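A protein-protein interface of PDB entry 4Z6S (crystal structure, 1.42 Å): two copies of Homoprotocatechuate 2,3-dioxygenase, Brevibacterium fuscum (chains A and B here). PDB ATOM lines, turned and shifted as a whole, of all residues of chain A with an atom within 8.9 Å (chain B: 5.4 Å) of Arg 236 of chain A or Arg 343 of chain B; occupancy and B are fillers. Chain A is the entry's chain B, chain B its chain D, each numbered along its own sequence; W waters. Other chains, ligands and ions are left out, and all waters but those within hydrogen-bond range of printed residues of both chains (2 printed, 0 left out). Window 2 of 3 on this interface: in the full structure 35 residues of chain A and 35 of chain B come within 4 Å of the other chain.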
ATOM      1  N   VAL A  38      -8.075  -7.417 -10.337  1.00  0.00           N
ATOM      2  CA  VAL A  38      -8.777  -8.498 -11.030  1.00  0.00           C
ATOM      3  C   VAL A  38      -7.788  -9.414 -11.740  1.00  0.00           C
ATOM      4  O   VAL A  38      -7.779 -10.619 -11.496  1.00  0.00           O
ATOM      5  CB  VAL A  38      -9.879  -7.980 -11.971  1.00  0.00           C
ATOM      6  CG1 VAL A  38     -10.567  -9.134 -12.686  1.00  0.00           C
ATOM      7  CG2 VAL A  38     -10.869  -7.156 -11.171  1.00  0.00           C
ATOM      8  N   CYS A 229     -12.475 -16.264 -15.762  1.00  0.00           N
ATOM      9  CA  CYS A 229     -13.926 -16.246 -15.932  1.00  0.00           C
ATOM     10  C   CYS A 229     -14.632 -16.431 -14.586  1.00  0.00           C
ATOM     11  O   CYS A 229     -15.548 -15.683 -14.255  1.00  0.00           O
ATOM     12  CB  CYS A 229     -14.357 -17.369 -16.885  1.00  0.00           C
ATOM     13  SG  CYS A 229     -13.725 -17.193 -18.574  1.00  0.00           S
ATOM     14  N   ASP A 230     -14.175 -17.425 -13.840  1.00  0.00           N
ATOM     15  CA  ASP A 230     -14.797 -17.761 -12.550  1.00  0.00           C
ATOM     16  C   ASP A 230     -14.680 -16.581 -11.587  1.00  0.00           C
ATOM     17  O   ASP A 230     -15.644 -16.261 -10.865  1.00  0.00           O
ATOM     18  CB  ASP A 230     -14.133 -19.002 -11.943  1.00  0.00           C
ATOM     19  CG  ASP A 230     -14.490 -20.304 -12.659  1.00  0.00           C
ATOM     20  OD1 ASP A 230     -15.578 -20.388 -13.298  1.00  0.00           O
ATOM     21  OD2 ASP A 230     -13.663 -21.257 -12.546  1.00  0.00           O
ATOM     22  N   LYS A 231     -13.515 -15.935 -11.570  1.00  0.00           N
ATOM     23  CA  LYS A 231     -13.281 -14.794 -10.663  1.00  0.00           C
ATOM     24  C   LYS A 231     -14.154 -13.612 -11.078  1.00  0.00           C
ATOM     25  O   LYS A 231     -14.721 -12.909 -10.238  1.00  0.00           O
ATOM     26  CB  LYS A 231     -11.818 -14.370 -10.700  1.00  0.00           C
ATOM     27  CG  LYS A 231     -11.494 -13.217  -9.775  1.00  0.00           C
ATOM     28  CD  LYS A 231      -9.987 -12.963  -9.727  1.00  0.00           C
ATOM     29  CE  LYS A 231      -9.630 -11.909  -8.702  1.00  0.00           C
ATOM     30  NZ  LYS A 231      -8.164 -11.613  -8.706  1.00  0.00           N
ATOM     31  N   MET A 232     -14.299 -13.397 -12.388  1.00  0.00           N
ATOM     32  CA  MET A 232     -15.162 -12.326 -12.837  1.00  0.00           C
ATOM     33  C   MET A 232     -16.627 -12.585 -12.480  1.00  0.00           C
ATOM     34  O   MET A 232     -17.358 -11.650 -12.130  1.00  0.00           O
ATOM     35  CB  MET A 232     -14.965 -12.091 -14.342  1.00  0.00           C
ATOM     36  CG  MET A 232     -13.611 -11.473 -14.635  1.00  0.00           C
ATOM     37  SD  MET A 232     -13.201 -11.186 -16.341  1.00  0.00           S
ATOM     38  CE  MET A 232     -14.189  -9.735 -16.643  1.00  0.00           C
ATOM     39  N   GLY A 233     -17.065 -13.836 -12.532  1.00  0.00           N
ATOM     40  CA  GLY A 233     -18.387 -14.179 -12.020  1.00  0.00           C
ATOM     41  C   GLY A 233     -18.508 -13.867 -10.531  1.00  0.00           C
ATOM     42  O   GLY A 233     -19.503 -13.286 -10.072  1.00  0.00           O
ATOM     43  N   ALA A 234     -17.495 -14.227  -9.768  1.00  0.00           N
ATOM     44  CA  ALA A 234     -17.546 -13.993  -8.318  1.00  0.00           C
ATOM     45  C   ALA A 234     -17.562 -12.503  -7.962  1.00  0.00           C
ATOM     46  O   ALA A 234     -18.166 -12.100  -6.974  1.00  0.00           O
ATOM     47  CB  ALA A 234     -16.398 -14.692  -7.657  1.00  0.00           C
ATOM     48  N   LEU A 235     -16.873 -11.691  -8.757  1.00  0.00           N
ATOM     49  CA  LEU A 235     -16.873 -10.258  -8.579  1.00  0.00           C
ATOM     50  C   LEU A 235     -18.108  -9.595  -9.205  1.00  0.00           C
ATOM     51  O   LEU A 235     -18.246  -8.372  -9.151  1.00  0.00           O
ATOM     52  CB  LEU A 235     -15.609  -9.692  -9.229  1.00  0.00           C
ATOM     53  CG  LEU A 235     -14.327 -10.033  -8.465  1.00  0.00           C
ATOM     54  CD1 LEU A 235     -13.103  -9.547  -9.237  1.00  0.00           C
ATOM     55  CD2 LEU A 235     -14.319  -9.426  -7.063  1.00  0.00           C
ATOM     56  N   ARG A 236     -18.982 -10.395  -9.822  1.00  0.00           N
ATOM     57  CA  ARG A 236     -20.217  -9.902 -10.436  1.00  0.00           C
ATOM     58  C   ARG A 236     -19.900  -8.852 -11.491  1.00  0.00           C
ATOM     59  O   ARG A 236     -20.599  -7.859 -11.629  1.00  0.00           O
ATOM     60  CB  ARG A 236     -21.208  -9.414  -9.376  1.00  0.00           C
ATOM     61  CG  ARG A 236     -21.893 -10.557  -8.652  1.00  0.00           C
ATOM     62  CD  ARG A 236     -23.065 -11.066  -9.440  1.00  0.00           C
ATOM     63  NE  ARG A 236     -23.633 -12.297  -8.872  1.00  0.00           N
ATOM     64  CZ  ARG A 236     -24.661 -12.942  -9.435  1.00  0.00           C
ATOM     65  NH1 ARG A 236     -25.275 -12.445 -10.502  1.00  0.00           N
ATOM     66  NH2 ARG A 236     -25.101 -14.099  -8.920  1.00  0.00           N
ATOM     67  N   ILE A 237     -18.889  -9.182 -12.297  1.00  0.00           N
ATOM     68  CA  ILE A 237     -18.525  -8.408 -13.492  1.00  0.00           C
ATOM     69  C   ILE A 237     -18.471  -9.281 -14.745  1.00  0.00           C
ATOM     70  O   ILE A 237     -17.684  -9.042 -15.675  1.00  0.00           O
ATOM     71  CB  ILE A 237     -17.212  -7.604 -13.280  1.00  0.00           C
ATOM     72  CG1 ILE A 237     -16.012  -8.523 -12.996  1.00  0.00           C
ATOM     73  CG2 ILE A 237     -17.399  -6.568 -12.192  1.00  0.00           C
ATOM     74  CD1 ILE A 237     -14.678  -7.835 -12.867  1.00  0.00           C
ATOM     75  N   SER A 238     -19.318 -10.316 -14.805  1.00  0.00           N
ATOM     76  CA  SER A 238     -19.382 -11.183 -15.978  1.00  0.00           C
ATOM     77  C   SER A 238     -19.840 -10.446 -17.227  1.00  0.00           C
ATOM     78  O   SER A 238     -19.595 -10.934 -18.340  1.00  0.00           O
ATOM     79  CB  SER A 238     -20.312 -12.383 -15.713  1.00  0.00           C
ATOM     80  OG  SER A 238     -21.627 -11.991 -15.396  1.00  0.00           O
ATOM     81  N   ASP A 239     -20.477  -9.282 -17.056  1.00  0.00           N
ATOM     82  CA  ASP A 239     -20.814  -8.435 -18.187  1.00  0.00           C
ATOM     83  C   ASP A 239     -19.582  -7.881 -18.901  1.00  0.00           C
ATOM     84  O   ASP A 239     -19.717  -7.343 -20.018  1.00  0.00           O
ATOM     85  CB  ASP A 239     -21.773  -7.297 -17.794  1.00  0.00           C
ATOM     86  CG  ASP A 239     -21.264  -6.411 -16.662  1.00  0.00           C
ATOM     87  OD1 ASP A 239     -20.605  -6.900 -15.723  1.00  0.00           O
ATOM     88  OD2 ASP A 239     -21.585  -5.189 -16.678  1.00  0.00           O
ATOM     89  N   ARG A 240     -18.401  -8.005 -18.282  1.00  0.00           N
ATOM     90  CA  ARG A 240     -17.168  -7.557 -18.883  1.00  0.00           C
ATOM     91  C   ARG A 240     -16.422  -8.692 -19.561  1.00  0.00           C
ATOM     92  O   ARG A 240     -15.319  -8.492 -20.086  1.00  0.00           O
ATOM     93  CB  ARG A 240     -16.273  -6.868 -17.831  1.00  0.00           C
ATOM     94  CG  ARG A 240     -17.000  -5.767 -17.051  1.00  0.00           C
ATOM     95  CD  ARG A 240     -17.717  -4.743 -17.934  1.00  0.00           C
ATOM     96  NE  ARG A 240     -16.739  -3.925 -18.654  1.00  0.00           N
ATOM     97  CZ  ARG A 240     -17.050  -3.065 -19.621  1.00  0.00           C
ATOM     98  NH1 ARG A 240     -18.275  -2.935 -20.031  1.00  0.00           N
ATOM     99  NH2 ARG A 240     -16.114  -2.337 -20.178  1.00  0.00           N
ATOM    100  N   ILE A 241     -16.999  -9.903 -19.536  1.00  0.00           N
ATOM    101  CA  ILE A 241     -16.565 -10.989 -20.392  1.00  0.00           C
ATOM    102  C   ILE A 241     -17.286 -10.821 -21.717  1.00  0.00           C
ATOM    103  O   ILE A 241     -18.497 -10.936 -21.779  1.00  0.00           O
ATOM    104  CB  ILE A 241     -16.871 -12.380 -19.789  1.00  0.00           C
ATOM    105  CG1 ILE A 241     -16.176 -12.561 -18.431  1.00  0.00           C
ATOM    106  CG2 ILE A 241     -16.542 -13.477 -20.799  1.00  0.00           C
ATOM    107  CD1 ILE A 241     -16.614 -13.823 -17.734  1.00  0.00           C
ATOM    108  N   TRP B 285     -31.831 -19.414  -6.562  1.00  0.00           N
ATOM    109  CA  TRP B 285     -31.443 -18.372  -7.486  1.00  0.00           C
ATOM    110  C   TRP B 285     -32.668 -17.711  -8.103  1.00  0.00           C
ATOM    111  O   TRP B 285     -33.677 -18.372  -8.360  1.00  0.00           O
ATOM    112  CB  TRP B 285     -30.633 -18.967  -8.629  1.00  0.00           C
ATOM    113  CG  TRP B 285     -29.360 -19.620  -8.256  1.00  0.00           C
ATOM    114  CD1 TRP B 285     -29.218 -20.807  -7.645  1.00  0.00           C
ATOM    115  CD2 TRP B 285     -28.031 -19.124  -8.474  1.00  0.00           C
ATOM    116  NE1 TRP B 285     -27.897 -21.104  -7.453  1.00  0.00           N
ATOM    117  CE2 TRP B 285     -27.140 -20.092  -7.973  1.00  0.00           C
ATOM    118  CE3 TRP B 285     -27.515 -17.958  -9.034  1.00  0.00           C
ATOM    119  CZ2 TRP B 285     -25.757 -19.923  -8.018  1.00  0.00           C
ATOM    120  CZ3 TRP B 285     -26.157 -17.819  -9.107  1.00  0.00           C
ATOM    121  CH2 TRP B 285     -25.295 -18.786  -8.580  1.00  0.00           C
ATOM    122  N   ASP B 289     -31.384 -13.786 -12.852  1.00  0.00           N
ATOM    123  CA  ASP B 289     -29.955 -13.686 -12.571  1.00  0.00           C
ATOM    124  C   ASP B 289     -29.208 -14.365 -13.738  1.00  0.00           C
ATOM    125  O   ASP B 289     -29.193 -15.590 -13.858  1.00  0.00           O
ATOM    126  CB  ASP B 289     -29.663 -14.395 -11.250  1.00  0.00           C
ATOM    127  CG  ASP B 289     -28.227 -14.252 -10.781  1.00  0.00           C
ATOM    128  OD1 ASP B 289     -27.341 -14.015 -11.651  1.00  0.00           O
ATOM    129  OD2 ASP B 289     -27.983 -14.390  -9.554  1.00  0.00           O
ATOM    130  N   ASN B 290     -28.514 -13.556 -14.524  1.00  0.00           N
ATOM    131  CA  ASN B 290     -27.783 -14.052 -15.691  1.00  0.00           C
ATOM    132  C   ASN B 290     -26.509 -14.858 -15.372  1.00  0.00           C
ATOM    133  O   ASN B 290     -25.858 -15.353 -16.293  1.00  0.00           O
ATOM    134  CB  ASN B 290     -27.426 -12.912 -16.638  1.00  0.00           C
ATOM    135  CG  ASN B 290     -26.975 -13.414 -18.001  1.00  0.00           C
ATOM    136  OD1 ASN B 290     -27.690 -14.151 -18.685  1.00  0.00           O
ATOM    137  ND2 ASN B 290     -25.779 -12.975 -18.423  1.00  0.00           N
ATOM    138  N   GLN B 291     -26.187 -15.031 -14.094  1.00  0.00           N
ATOM    139  CA  GLN B 291     -25.099 -15.944 -13.707  1.00  0.00           C
ATOM    140  C   GLN B 291     -25.608 -17.285 -13.145  1.00  0.00           C
ATOM    141  O   GLN B 291     -24.802 -18.112 -12.695  1.00  0.00           O
ATOM    142  CB  GLN B 291     -24.147 -15.270 -12.691  1.00  0.00           C
ATOM    143  CG  GLN B 291     -23.402 -14.078 -13.301  1.00  0.00           C
ATOM    144  CD  GLN B 291     -22.310 -13.449 -12.464  1.00  0.00           C
ATOM    145  OE1 GLN B 291     -21.755 -12.409 -12.847  1.00  0.00           O
ATOM    146  NE2 GLN B 291     -21.995 -14.037 -11.332  1.00  0.00           N
ATOM    147  N   TRP B 295     -22.369 -19.152 -15.132  1.00  0.00           N
ATOM    148  CA  TRP B 295     -21.782 -18.219 -14.167  1.00  0.00           C
ATOM    149  C   TRP B 295     -21.030 -17.050 -14.847  1.00  0.00           C
ATOM    150  O   TRP B 295     -20.872 -15.993 -14.254  1.00  0.00           O
ATOM    151  CB  TRP B 295     -20.807 -19.028 -13.352  1.00  0.00           C
ATOM    152  CG  TRP B 295     -20.065 -18.338 -12.225  1.00  0.00           C
ATOM    153  CD1 TRP B 295     -18.725 -18.257 -12.094  1.00  0.00           C
ATOM    154  CD2 TRP B 295     -20.618 -17.724 -11.056  1.00  0.00           C
ATOM    155  NE1 TRP B 295     -18.389 -17.638 -10.931  1.00  0.00           N
ATOM    156  CE2 TRP B 295     -19.533 -17.306 -10.254  1.00  0.00           C
ATOM    157  CE3 TRP B 295     -21.926 -17.509 -10.593  1.00  0.00           C
ATOM    158  CZ2 TRP B 295     -19.704 -16.665  -9.024  1.00  0.00           C
ATOM    159  CZ3 TRP B 295     -22.088 -16.857  -9.357  1.00  0.00           C
ATOM    160  CH2 TRP B 295     -20.993 -16.447  -8.594  1.00  0.00           C
ATOM    161  N   PHE B 341     -30.221  -9.865 -15.511  1.00  0.00           N
ATOM    162  CA  PHE B 341     -29.273  -8.927 -14.909  1.00  0.00           C
ATOM    163  C   PHE B 341     -27.935  -9.587 -14.617  1.00  0.00           C
ATOM    164  O   PHE B 341     -27.860 -10.806 -14.413  1.00  0.00           O
ATOM    165  CB  PHE B 341     -29.831  -8.279 -13.627  1.00  0.00           C
ATOM    166  CG  PHE B 341     -30.109  -9.258 -12.497  1.00  0.00           C
ATOM    167  CD1 PHE B 341     -29.091  -9.731 -11.667  1.00  0.00           C
ATOM    168  CD2 PHE B 341     -31.404  -9.690 -12.256  1.00  0.00           C
ATOM    169  CE1 PHE B 341     -29.358 -10.602 -10.617  1.00  0.00           C
ATOM    170  CE2 PHE B 341     -31.668 -10.584 -11.220  1.00  0.00           C
ATOM    171  CZ  PHE B 341     -30.654 -11.021 -10.386  1.00  0.00           C
ATOM    172  N   THR B 342     -26.887  -8.770 -14.532  1.00  0.00           N
ATOM    173  CA  THR B 342     -25.612  -9.218 -13.965  1.00  0.00           C
ATOM    174  C   THR B 342     -25.551  -8.944 -12.459  1.00  0.00           C
ATOM    175  O   THR B 342     -25.135  -9.797 -11.688  1.00  0.00           O
ATOM    176  CB  THR B 342     -24.418  -8.539 -14.665  1.00  0.00           C
ATOM    177  OG1 THR B 342     -24.466  -8.810 -16.075  1.00  0.00           O
ATOM    178  CG2 THR B 342     -23.113  -9.039 -14.131  1.00  0.00           C
ATOM    179  N   ARG B 343     -25.951  -7.732 -12.078  1.00  0.00           N
ATOM    180  CA  ARG B 343     -26.079  -7.334 -10.670  1.00  0.00           C
ATOM    181  C   ARG B 343     -27.521  -6.937 -10.421  1.00  0.00           C
ATOM    182  O   ARG B 343     -28.073  -6.118 -11.175  1.00  0.00           O
ATOM    183  CB  ARG B 343     -25.157  -6.163 -10.355  1.00  0.00           C
ATOM    184  CG  ARG B 343     -23.673  -6.488 -10.479  1.00  0.00           C
ATOM    185  CD  ARG B 343     -22.827  -5.226 -10.664  1.00  0.00           C
ATOM    186  NE  ARG B 343     -23.096  -4.569 -11.935  1.00  0.00           N
ATOM    187  CZ  ARG B 343     -22.521  -4.867 -13.096  1.00  0.00           C
ATOM    188  NH1 ARG B 343     -21.600  -5.813 -13.198  1.00  0.00           N
ATOM    189  NH2 ARG B 343     -22.878  -4.205 -14.186  1.00  0.00           N
ATOM    190  N   ALA B 344     -28.139  -7.528  -9.397  1.00  0.00           N
ATOM    191  CA  ALA B 344     -29.549  -7.277  -9.138  1.00  0.00           C
ATOM    192  C   ALA B 344     -29.767  -5.788  -8.920  1.00  0.00           C
ATOM    193  O   ALA B 344     -29.026  -5.140  -8.183  1.00  0.00           O
ATOM    194  CB  ALA B 344     -30.040  -8.072  -7.936  1.00  0.00           C
ATOM    195  N   GLY B 345     -30.760  -5.264  -9.628  1.00  0.00           N
ATOM    196  CA  GLY B 345     -31.082  -3.851  -9.563  1.00  0.00           C
ATOM    197  C   GLY B 345     -30.250  -2.890 -10.395  1.00  0.00           C
ATOM    198  O   GLY B 345     -30.521  -1.688 -10.385  1.00  0.00           O
ATOM    199  N   ASP B 346     -29.251  -3.399 -11.125  1.00  0.00           N
ATOM    200  CA  ASP B 346     -28.364  -2.541 -11.935  1.00  0.00           C
ATOM    201  C   ASP B 346     -28.774  -2.667 -13.379  1.00  0.00           C
ATOM    202  O   ASP B 346     -28.815  -3.769 -13.912  1.00  0.00           O
ATOM    203  CB  ASP B 346     -26.911  -2.976 -11.767  1.00  0.00           C
ATOM    204  CG  ASP B 346     -25.926  -1.995 -12.321  1.00  0.00           C
ATOM    205  OD1 ASP B 346     -26.312  -0.988 -12.964  1.00  0.00           O
ATOM    206  OD2 ASP B 346     -24.730  -2.264 -12.133  1.00  0.00           O
ATOM    207  N   ASP B 348     -26.939  -1.413 -15.793  1.00  0.00           N
ATOM    208  CA  ASP B 348     -25.677  -1.737 -16.461  1.00  0.00           C
ATOM    209  C   ASP B 348     -25.469  -3.230 -16.370  1.00  0.00           C
ATOM    210  O   ASP B 348     -25.550  -3.802 -15.291  1.00  0.00           O
ATOM    211  CB  ASP B 348     -24.477  -1.069 -15.811  1.00  0.00           C
ATOM    212  CG  ASP B 348     -24.501   0.439 -15.897  1.00  0.00           C
ATOM    213  OD1 ASP B 348     -25.131   0.968 -16.834  1.00  0.00           O
ATOM    214  OD2 ASP B 348     -23.862   1.085 -15.033  1.00  0.00           O
ATOM    215  N   GLY B 349     -25.215  -3.869 -17.500  1.00  0.00           N
ATOM    216  CA  GLY B 349     -25.037  -5.312 -17.528  1.00  0.00           C
ATOM    217  C   GLY B 349     -26.324  -6.080 -17.481  1.00  0.00           C
ATOM    218  O   GLY B 349     -26.313  -7.288 -17.226  1.00  0.00           O
HETATM  219  O   HOH W   1     -19.593  -3.754 -15.010  1.00  0.00           O
HETATM  220  O   HOH W   2     -23.789 -11.388 -16.993  1.00  0.00           O
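The backbone carbonyl oxygen of Asp 230 of chain A sits at hydrogen-bond distance from the indole nitrogen of Trp 295 of chain B, at 3.1 Å. The side-chain amide nitrogen (NE2) of Gln 291 of chain B is in hydrogen-bond range of the backbone carbonyl oxygen (O) of Gly 233 of chain A, 2.9 Å away. The guanidinium group of Arg 236 of chain A lies within salt-bridge range of the side-chain carboxylate of Asp 289 of chain B (2.8 Å). NE of Arg 236 of chain A lies close to NE2 of Gln 291 of chain B (3.4 Å). The backbone carbonyl oxygen of Thr 342 of chain B lies within hydrogen-bond range of the guanidinium group of Arg 236 of chain A, at 2.9 Å. The guanidinium group (NH1) of Arg 343 of chain B is in hydrogen-bond range of the backbone carbonyl oxygen (O) of Arg 236 of chain A. The side-chain amide oxygen (OE1) of Gln 291 of chain B lies within hydrogen-bond range of the side-chain hydroxyl (OG) of Ser 238 of chain A (2.6 Å). The side-chain carboxylate (OD1) of Asp 239 of chain A lies within salt-bridge range of the guanidinium group (NH1) of Arg 343 of chain B (2.9 Å).
OD1 of Asp 289 of chain B lies within hydrogen-bond range of N of Gln 291 of chain B. O of Gly 349 of chain B sits at hydrogen-bond distance from OG1 of Thr 342 of chain B (2.7 Å). OD2 of Asp 346 of chain B lies within salt-bridge range of NE of Arg 343 of chain B (2.8 Å). The backbone carbonyl oxygen (O) of Asp 348 of chain B lies within hydrogen-bond range of the guanidinium group (NH2) of Arg 343 of chain B (2.9 Å).
Among the printed residues, pairs that only touch across the chains: Gly 233 of chain A with Trp 295 of chain B (3.4 Å), Ala 234 of chain A with Trp 295 of chain B (3.4 Å), Arg 236 of chain A with Trp 285 of chain B (3.9 Å), Ser 238 of chain A with Trp 295 of chain B (3.9 Å), Ser 238 of chain A with Thr 342 of chain B (3.5 Å), Asp 239 of chain A with Thr 342 of chain B (3.5 Å) and Asp 239 of chain A with Gly 349 of chain B (3.6 Å).
Arg 236 of chain A touches five residues of chain B. Arg 343 of chain B touches just these residues of chain A: Arg 236 (2.8 Å) and Asp 239 (2.9 Å). No residue of chain A comes within 4 Å of Ala 344 of chain B. Of the printed residues of chain B, Asp 230 of chain A touches Trp 295. Of the printed residues of chain A, Gln 291 of chain B touches Gly 233, Arg 236 and Ser 238. Printed residues of chain A within 4 Å of Trp 295 of chain B: Asp 230, Gly 233, Ala 234 and Ser 238. Of the printed residues of chain A, Trp 285 of chain B touches Arg 236 (3.9 Å). Printed residues of chain A within 4 Å of Gly 349 of chain B: Asp 239. Asp 348 of chain B touches none of the printed residues of chain A. Asn 290 of chain B touches none of the printed residues of chain A. The nearest residue of chain B that does not touch Arg 236 of chain A is Trp 295 of chain B (4.1 Å). The nearest residue of chain A that does not touch Arg 343 of chain B is Ile 237 of chain A (4.03 Å).
Of the 13 printed residues of chain B, 7 touch a printed residue of chain A. Hydrophobic or aromatic side chains of chain B that line the printed part of chain A: Trp 285 and Trp 295.
No position is printed for both chains.
Water W2 lies within hydrogen-bond range of OG of Ser 238 of chain A (2.8 Å), OG1 of Thr 342 of chain B (2.8 Å) and ND2 of Asn 290 of chain B (2.9 Å). Water W1 lies within hydrogen-bond range of OD2 of Asp 239 of chain A (3.0 Å) and NH1 of Arg 343 of chain B (3.4 Å).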
